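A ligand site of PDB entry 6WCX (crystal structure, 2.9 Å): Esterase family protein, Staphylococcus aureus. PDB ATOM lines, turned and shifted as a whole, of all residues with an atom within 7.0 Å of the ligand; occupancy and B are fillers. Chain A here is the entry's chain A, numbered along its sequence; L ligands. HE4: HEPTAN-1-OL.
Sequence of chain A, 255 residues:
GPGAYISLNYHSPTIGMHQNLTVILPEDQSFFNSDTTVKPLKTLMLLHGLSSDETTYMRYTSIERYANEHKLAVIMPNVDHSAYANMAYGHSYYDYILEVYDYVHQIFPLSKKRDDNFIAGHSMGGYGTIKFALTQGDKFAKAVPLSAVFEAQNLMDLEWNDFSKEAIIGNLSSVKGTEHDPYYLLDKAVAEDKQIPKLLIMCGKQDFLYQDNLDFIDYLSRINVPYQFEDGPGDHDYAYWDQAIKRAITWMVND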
ATOM      1  N   HIS A  48     -15.712  -3.151 -18.579  1.00  0.00           N
ATOM      2  CA  HIS A  48     -16.869  -2.278 -18.439  1.00  0.00           C
ATOM      3  C   HIS A  48     -18.145  -3.072 -18.203  1.00  0.00           C
ATOM      4  O   HIS A  48     -18.207  -4.288 -18.421  1.00  0.00           O
ATOM      5  CB  HIS A  48     -17.033  -1.419 -19.680  1.00  0.00           C
ATOM      6  CG  HIS A  48     -17.314  -2.203 -20.915  1.00  0.00           C
ATOM      7  ND1 HIS A  48     -18.580  -2.609 -21.271  1.00  0.00           N
ATOM      8  CD2 HIS A  48     -16.487  -2.656 -21.892  1.00  0.00           C
ATOM      9  CE1 HIS A  48     -18.519  -3.286 -22.413  1.00  0.00           C
ATOM     10  NE2 HIS A  48     -17.260  -3.329 -22.800  1.00  0.00           N
ATOM     11  N   GLY A  49     -19.204  -2.350 -17.803  1.00  0.00           N
ATOM     12  CA  GLY A  49     -20.510  -2.931 -17.604  1.00  0.00           C
ATOM     13  C   GLY A  49     -21.404  -2.779 -18.822  1.00  0.00           C
ATOM     14  O   GLY A  49     -20.966  -2.329 -19.886  1.00  0.00           O
ATOM     15  N   LEU A  50     -22.662  -3.180 -18.669  1.00  0.00           N
ATOM     16  CA  LEU A  50     -23.623  -3.075 -19.764  1.00  0.00           C
ATOM     17  C   LEU A  50     -23.891  -1.620 -20.127  1.00  0.00           C
ATOM     18  O   LEU A  50     -23.934  -0.750 -19.263  1.00  0.00           O
ATOM     19  CB  LEU A  50     -24.944  -3.758 -19.391  1.00  0.00           C
ATOM     20  CG  LEU A  50     -25.908  -4.015 -20.554  1.00  0.00           C
ATOM     21  CD1 LEU A  50     -25.243  -4.856 -21.625  1.00  0.00           C
ATOM     22  CD2 LEU A  50     -27.195  -4.700 -20.083  1.00  0.00           C
ATOM     23  N   SER A  51     -24.010  -1.375 -21.443  1.00  0.00           N
ATOM     24  CA  SER A  51     -24.272  -0.119 -22.178  1.00  0.00           C
ATOM     25  C   SER A  51     -22.989   0.688 -22.349  1.00  0.00           C
ATOM     26  O   SER A  51     -23.031   1.741 -23.009  1.00  0.00           O
ATOM     27  CB  SER A  51     -25.371   0.771 -21.575  1.00  0.00           C
ATOM     28  OG  SER A  51     -25.026   1.255 -20.299  1.00  0.00           O
ATOM     29  N   HIS A 122     -17.038  -3.462 -13.321  1.00  0.00           N
ATOM     30  CA  HIS A 122     -18.293  -3.108 -12.661  1.00  0.00           C
ATOM     31  C   HIS A 122     -19.502  -3.708 -13.374  1.00  0.00           C
ATOM     32  O   HIS A 122     -19.518  -3.833 -14.599  1.00  0.00           O
ATOM     33  CB  HIS A 122     -18.465  -1.593 -12.524  1.00  0.00           C
ATOM     34  CG  HIS A 122     -18.817  -0.897 -13.799  1.00  0.00           C
ATOM     35  ND1 HIS A 122     -17.854  -0.375 -14.639  1.00  0.00           N
ATOM     36  CD2 HIS A 122     -20.005  -0.634 -14.376  1.00  0.00           C
ATOM     37  CE1 HIS A 122     -18.439   0.184 -15.677  1.00  0.00           C
ATOM     38  NE2 HIS A 122     -19.743   0.036 -15.549  1.00  0.00           N
ATOM     39  N   SER A 123     -20.513  -4.071 -12.561  1.00  0.00           N
ATOM     40  CA  SER A 123     -21.796  -4.630 -13.005  1.00  0.00           C
ATOM     41  C   SER A 123     -21.605  -5.876 -13.869  1.00  0.00           C
ATOM     42  O   SER A 123     -21.265  -6.946 -13.348  1.00  0.00           O
ATOM     43  CB  SER A 123     -22.620  -3.576 -13.741  1.00  0.00           C
ATOM     44  OG  SER A 123     -23.827  -4.117 -14.253  1.00  0.00           O
ATOM     45  N   MET A 124     -21.836  -5.747 -15.166  1.00  0.00           N
ATOM     46  CA  MET A 124     -21.532  -6.830 -16.089  1.00  0.00           C
ATOM     47  C   MET A 124     -20.042  -7.098 -16.169  1.00  0.00           C
ATOM     48  O   MET A 124     -19.629  -8.252 -16.387  1.00  0.00           O
ATOM     49  CB  MET A 124     -22.105  -6.507 -17.467  1.00  0.00           C
ATOM     50  CG  MET A 124     -21.911  -7.555 -18.511  1.00  0.00           C
ATOM     51  SD  MET A 124     -22.396  -6.904 -20.111  1.00  0.00           S
ATOM     52  CE  MET A 124     -20.940  -5.980 -20.559  1.00  0.00           C
ATOM     53  N   GLY A 125     -19.208  -6.055 -16.010  1.00  0.00           N
ATOM     54  CA  GLY A 125     -17.780  -6.260 -15.879  1.00  0.00           C
ATOM     55  C   GLY A 125     -17.392  -6.988 -14.616  1.00  0.00           C
ATOM     56  O   GLY A 125     -16.387  -7.694 -14.590  1.00  0.00           O
ATOM     57  N   GLY A 126     -18.163  -6.808 -13.537  1.00  0.00           N
ATOM     58  CA  GLY A 126     -17.944  -7.604 -12.340  1.00  0.00           C
ATOM     59  C   GLY A 126     -18.315  -9.066 -12.564  1.00  0.00           C
ATOM     60  O   GLY A 126     -17.716  -9.962 -11.954  1.00  0.00           O
ATOM     61  N   SER A 147     -19.731  -3.705  -7.613  1.00  0.00           N
ATOM     62  CA  SER A 147     -21.178  -3.584  -7.815  1.00  0.00           C
ATOM     63  C   SER A 147     -21.723  -4.710  -8.700  1.00  0.00           C
ATOM     64  O   SER A 147     -22.545  -4.480  -9.608  1.00  0.00           O
ATOM     65  CB  SER A 147     -21.548  -2.217  -8.392  1.00  0.00           C
ATOM     66  OG  SER A 147     -22.898  -2.176  -8.824  1.00  0.00           O
ATOM     67  N   ALA A 148     -21.167  -5.903  -8.542  1.00  0.00           N
ATOM     68  CA  ALA A 148     -21.217  -6.946  -9.540  1.00  0.00           C
ATOM     69  C   ALA A 148     -22.548  -7.711  -9.601  1.00  0.00           C
ATOM     70  O   ALA A 148     -23.391  -7.649  -8.697  1.00  0.00           O
ATOM     71  CB  ALA A 148     -20.089  -7.945  -9.291  1.00  0.00           C
ATOM     72  N   VAL A 149     -22.702  -8.435 -10.714  1.00  0.00           N
ATOM     73  CA  VAL A 149     -23.663  -9.519 -10.927  1.00  0.00           C
ATOM     74  C   VAL A 149     -23.019 -10.897 -10.723  1.00  0.00           C
ATOM     75  O   VAL A 149     -21.985 -11.229 -11.316  1.00  0.00           O
ATOM     76  CB  VAL A 149     -24.408  -9.382 -12.274  1.00  0.00           C
ATOM     77  CG1 VAL A 149     -24.911 -10.757 -12.884  1.00  0.00           C
ATOM     78  CG2 VAL A 149     -25.701  -8.634 -11.969  1.00  0.00           C
ATOM     79  N   GLU A 151     -25.563 -13.617  -9.451  1.00  0.00           N
ATOM     80  CA  GLU A 151     -26.680 -14.479  -9.837  1.00  0.00           C
ATOM     81  C   GLU A 151     -26.978 -14.172 -11.299  1.00  0.00           C
ATOM     82  O   GLU A 151     -27.526 -13.121 -11.617  1.00  0.00           O
ATOM     83  CB  GLU A 151     -27.898 -14.241  -8.940  1.00  0.00           C
ATOM     84  CG  GLU A 151     -29.150 -14.969  -9.377  1.00  0.00           C
ATOM     85  CD  GLU A 151     -28.861 -16.400  -9.781  1.00  0.00           C
ATOM     86  OE1 GLU A 151     -28.902 -16.694 -11.001  1.00  0.00           O
ATOM     87  OE2 GLU A 151     -28.558 -17.215  -8.881  1.00  0.00           O
ATOM     88  N   GLN A 153     -29.019 -15.200 -13.497  1.00  0.00           N
ATOM     89  CA  GLN A 153     -30.377 -15.073 -14.011  1.00  0.00           C
ATOM     90  C   GLN A 153     -30.853 -13.630 -13.994  1.00  0.00           C
ATOM     91  O   GLN A 153     -31.694 -13.240 -14.817  1.00  0.00           O
ATOM     92  CB  GLN A 153     -31.341 -15.949 -13.216  1.00  0.00           C
ATOM     93  CG  GLN A 153     -31.486 -17.366 -13.772  1.00  0.00           C
ATOM     94  CD  GLN A 153     -32.058 -17.398 -15.186  1.00  0.00           C
ATOM     95  OE1 GLN A 153     -31.527 -18.093 -16.066  1.00  0.00           O
ATOM     96  NE2 GLN A 153     -33.168 -16.684 -15.403  1.00  0.00           N
ATOM     97  N   ASN A 154     -30.321 -12.814 -13.068  1.00  0.00           N
ATOM     98  CA  ASN A 154     -30.761 -11.428 -12.966  1.00  0.00           C
ATOM     99  C   ASN A 154     -30.281 -10.591 -14.149  1.00  0.00           C
ATOM    100  O   ASN A 154     -30.954  -9.635 -14.535  1.00  0.00           O
ATOM    101  CB  ASN A 154     -30.276 -10.817 -11.658  1.00  0.00           C
ATOM    102  CG  ASN A 154     -30.748 -11.597 -10.442  1.00  0.00           C
ATOM    103  OD1 ASN A 154     -31.599 -12.493 -10.551  1.00  0.00           O
ATOM    104  ND2 ASN A 154     -30.202 -11.264  -9.273  1.00  0.00           N
ATOM    105  N   LEU A 155     -29.130 -10.952 -14.734  1.00  0.00           N
ATOM    106  CA  LEU A 155     -28.626 -10.263 -15.904  1.00  0.00           C
ATOM    107  C   LEU A 155     -29.234 -10.799 -17.197  1.00  0.00           C
ATOM    108  O   LEU A 155     -29.542 -10.008 -18.092  1.00  0.00           O
ATOM    109  CB  LEU A 155     -27.103 -10.373 -15.940  1.00  0.00           C
ATOM    110  CG  LEU A 155     -26.353  -9.909 -17.180  1.00  0.00           C
ATOM    111  CD1 LEU A 155     -26.356  -8.403 -17.287  1.00  0.00           C
ATOM    112  CD2 LEU A 155     -24.942 -10.413 -17.078  1.00  0.00           C
ATOM    113  N   MET A 156     -29.445 -12.123 -17.285  1.00  0.00           N
ATOM    114  CA  MET A 156     -30.066 -12.702 -18.472  1.00  0.00           C
ATOM    115  C   MET A 156     -31.515 -12.268 -18.617  1.00  0.00           C
ATOM    116  O   MET A 156     -31.967 -11.965 -19.725  1.00  0.00           O
ATOM    117  CB  MET A 156     -29.995 -14.235 -18.454  1.00  0.00           C
ATOM    118  CG  MET A 156     -28.602 -14.838 -18.426  1.00  0.00           C
ATOM    119  SD  MET A 156     -27.427 -14.096 -19.575  1.00  0.00           S
ATOM    120  CE  MET A 156     -25.911 -14.917 -19.129  1.00  0.00           C
ATOM    121  N   LEU A 158     -32.686  -9.443 -17.537  1.00  0.00           N
ATOM    122  CA  LEU A 158     -32.772  -7.992 -17.428  1.00  0.00           C
ATOM    123  C   LEU A 158     -33.401  -7.382 -18.675  1.00  0.00           C
ATOM    124  O   LEU A 158     -33.090  -7.772 -19.803  1.00  0.00           O
ATOM    125  CB  LEU A 158     -31.380  -7.404 -17.180  1.00  0.00           C
ATOM    126  CG  LEU A 158     -31.184  -5.906 -17.411  1.00  0.00           C
ATOM    127  CD1 LEU A 158     -32.003  -5.060 -16.431  1.00  0.00           C
ATOM    128  CD2 LEU A 158     -29.701  -5.563 -17.340  1.00  0.00           C
ATOM    129  N   TRP A 160     -33.028  -4.438 -20.249  1.00  0.00           N
ATOM    130  CA  TRP A 160     -32.283  -3.252 -20.615  1.00  0.00           C
ATOM    131  C   TRP A 160     -32.512  -2.953 -22.099  1.00  0.00           C
ATOM    132  O   TRP A 160     -32.856  -3.853 -22.875  1.00  0.00           O
ATOM    133  CB  TRP A 160     -30.786  -3.430 -20.320  1.00  0.00           C
ATOM    134  CG  TRP A 160     -29.967  -2.158 -20.352  1.00  0.00           C
ATOM    135  CD1 TRP A 160     -29.012  -1.812 -21.276  1.00  0.00           C
ATOM    136  CD2 TRP A 160     -30.043  -1.056 -19.426  1.00  0.00           C
ATOM    137  NE1 TRP A 160     -28.485  -0.575 -20.985  1.00  0.00           N
ATOM    138  CE2 TRP A 160     -29.094  -0.084 -19.852  1.00  0.00           C
ATOM    139  CE3 TRP A 160     -30.811  -0.787 -18.294  1.00  0.00           C
ATOM    140  CZ2 TRP A 160     -28.908   1.116 -19.178  1.00  0.00           C
ATOM    141  CZ3 TRP A 160     -30.625   0.399 -17.624  1.00  0.00           C
ATOM    142  CH2 TRP A 160     -29.677   1.346 -18.066  1.00  0.00           C
ATOM    143  N   ASP A 207     -27.348   0.142  -3.983  1.00  0.00           N
ATOM    144  CA  ASP A 207     -27.408  -0.527  -5.283  1.00  0.00           C
ATOM    145  C   ASP A 207     -28.484  -1.594  -5.278  1.00  0.00           C
ATOM    146  O   ASP A 207     -28.789  -2.181  -4.236  1.00  0.00           O
ATOM    147  CB  ASP A 207     -26.047  -1.153  -5.630  1.00  0.00           C
ATOM    148  CG  ASP A 207     -25.844  -1.371  -7.137  1.00  0.00           C
ATOM    149  OD1 ASP A 207     -26.710  -1.970  -7.795  1.00  0.00           O
ATOM    150  OD2 ASP A 207     -24.794  -0.925  -7.665  1.00  0.00           O
ATOM    151  N   PHE A 208     -29.064  -1.853  -6.455  1.00  0.00           N
ATOM    152  CA  PHE A 208     -29.995  -2.959  -6.605  1.00  0.00           C
ATOM    153  C   PHE A 208     -29.328  -4.286  -6.309  1.00  0.00           C
ATOM    154  O   PHE A 208     -29.920  -5.176  -5.685  1.00  0.00           O
ATOM    155  CB  PHE A 208     -30.582  -2.978  -8.013  1.00  0.00           C
ATOM    156  CG  PHE A 208     -31.417  -4.212  -8.312  1.00  0.00           C
ATOM    157  CD1 PHE A 208     -31.130  -5.011  -9.412  1.00  0.00           C
ATOM    158  CD2 PHE A 208     -32.486  -4.577  -7.501  1.00  0.00           C
ATOM    159  CE1 PHE A 208     -31.884  -6.144  -9.698  1.00  0.00           C
ATOM    160  CE2 PHE A 208     -33.238  -5.713  -7.778  1.00  0.00           C
ATOM    161  CZ  PHE A 208     -32.931  -6.487  -8.885  1.00  0.00           C
ATOM    162  N   LEU A 209     -28.065  -4.428  -6.710  1.00  0.00           N
ATOM    163  CA  LEU A 209     -27.323  -5.671  -6.571  1.00  0.00           C
ATOM    164  C   LEU A 209     -26.601  -5.811  -5.242  1.00  0.00           C
ATOM    165  O   LEU A 209     -25.681  -6.623  -5.146  1.00  0.00           O
ATOM    166  CB  LEU A 209     -26.320  -5.815  -7.715  1.00  0.00           C
ATOM    167  CG  LEU A 209     -26.921  -5.659  -9.099  1.00  0.00           C
ATOM    168  CD1 LEU A 209     -25.852  -5.654 -10.164  1.00  0.00           C
ATOM    169  CD2 LEU A 209     -27.886  -6.820  -9.320  1.00  0.00           C
ATOM    170  N   ASP A 212     -27.772  -9.087  -3.958  1.00  0.00           N
ATOM    171  CA  ASP A 212     -27.101 -10.055  -4.811  1.00  0.00           C
ATOM    172  C   ASP A 212     -25.650 -10.260  -4.382  1.00  0.00           C
ATOM    173  O   ASP A 212     -25.153 -11.392  -4.388  1.00  0.00           O
ATOM    174  CB  ASP A 212     -27.150  -9.597  -6.272  1.00  0.00           C
ATOM    175  CG  ASP A 212     -26.885 -10.720  -7.241  1.00  0.00           C
ATOM    176  OD1 ASP A 212     -25.743 -11.229  -7.289  1.00  0.00           O
ATOM    177  OD2 ASP A 212     -27.835 -11.109  -7.960  1.00  0.00           O
ATOM    178  N   HIS A 236     -25.586   2.655  -8.148  1.00  0.00           N
ATOM    179  CA  HIS A 236     -25.133   2.032  -9.385  1.00  0.00           C
ATOM    180  C   HIS A 236     -24.810   3.126 -10.409  1.00  0.00           C
ATOM    181  O   HIS A 236     -25.513   3.322 -11.404  1.00  0.00           O
ATOM    182  CB  HIS A 236     -26.186   1.073  -9.928  1.00  0.00           C
ATOM    183  CG  HIS A 236     -25.634  -0.002 -10.801  1.00  0.00           C
ATOM    184  ND1 HIS A 236     -25.199  -1.213 -10.319  1.00  0.00           N
ATOM    185  CD2 HIS A 236     -25.398  -0.021 -12.139  1.00  0.00           C
ATOM    186  CE1 HIS A 236     -24.758  -1.961 -11.314  1.00  0.00           C
ATOM    187  NE2 HIS A 236     -24.862  -1.254 -12.435  1.00  0.00           N
ATOM    188  N   TRP A 241     -18.248   4.168  -8.799  1.00  0.00           N
ATOM    189  CA  TRP A 241     -17.160   3.383  -9.385  1.00  0.00           C
ATOM    190  C   TRP A 241     -15.891   4.203  -9.551  1.00  0.00           C
ATOM    191  O   TRP A 241     -14.800   3.618  -9.590  1.00  0.00           O
ATOM    192  CB  TRP A 241     -17.595   2.799 -10.735  1.00  0.00           C
ATOM    193  CG  TRP A 241     -18.816   1.949 -10.594  1.00  0.00           C
ATOM    194  CD1 TRP A 241     -19.087   1.097  -9.569  1.00  0.00           C
ATOM    195  CD2 TRP A 241     -19.940   1.896 -11.476  1.00  0.00           C
ATOM    196  NE1 TRP A 241     -20.309   0.508  -9.769  1.00  0.00           N
ATOM    197  CE2 TRP A 241     -20.850   0.984 -10.938  1.00  0.00           C
ATOM    198  CE3 TRP A 241     -20.251   2.531 -12.679  1.00  0.00           C
ATOM    199  CZ2 TRP A 241     -22.061   0.679 -11.547  1.00  0.00           C
ATOM    200  CZ3 TRP A 241     -21.449   2.241 -13.288  1.00  0.00           C
ATOM    201  CH2 TRP A 241     -22.340   1.322 -12.722  1.00  0.00           C
HETATM  202  CAA HE4 L   1     -28.986  -7.289 -13.125  1.00  0.00           C
HETATM  203  CAC HE4 L   1     -28.622  -5.840 -12.852  1.00  0.00           C
HETATM  204  CAE HE4 L   1     -27.818  -5.363 -14.055  1.00  0.00           C
HETATM  205  CAG HE4 L   1     -27.545  -3.858 -14.015  1.00  0.00           C
HETATM  206  CAH HE4 L   1     -27.076  -3.388 -15.390  1.00  0.00           C
HETATM  207  CAF HE4 L   1     -25.636  -2.882 -15.304  1.00  0.00           C
HETATM  208  CAD HE4 L   1     -24.682  -4.072 -15.327  1.00  0.00           C
HETATM  209  OAB HE4 L   1     -23.752  -3.926 -16.359  1.00  0.00           O
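The backbone NH of Met 124 is in hydrogen-bond range of an oxygen (OAB) of the ligand (2.9 Å). CAD of the ligand is bonded to OG of Ser 123, 1.4 Å away. The backbone NH of Leu 50 is in hydrogen-bond range of an oxygen (OAB) of the ligand, 2.7 Å away.
ND2 of Asn 154 is in hydrogen-bond range of OD2 of Asp 212, at 2.7 Å. N of Val 149 sits at hydrogen-bond distance from O of Ser 123. N of Gly 49 lies within hydrogen-bond range of NE2 of His 122 (3.3 Å). A ring nitrogen (ND1) of His 236 sits at hydrogen-bond distance from the side-chain hydroxyl (OG) of Ser 147 (2.9 Å). OD2 of Asp 207 is in hydrogen-bond range of ND1 of His 236 (2.7 Å). N of Leu 209 lies within hydrogen-bond range of OD1 of Asp 207 (3.0 Å).
Gly 49 touches the ligand. Val 149 touches the ligand. O of Asn 154 touches CAA of the ligand, at 3.4 Å. Leu 158 touches the ligand (CD2 to CAE, 3.8 Å). CD2 of Leu 209 touches CAC of the ligand, at 3.7 Å. His 236 touches the ligand. Within 4 Å of the ligand: Gly 49, Leu 50, Ser 123, Met 124, Val 149, Asn 154, Leu 158, Leu 209 and His 236. Along chain A the residues within 4 Å of the ligand span positions 49 to 236.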
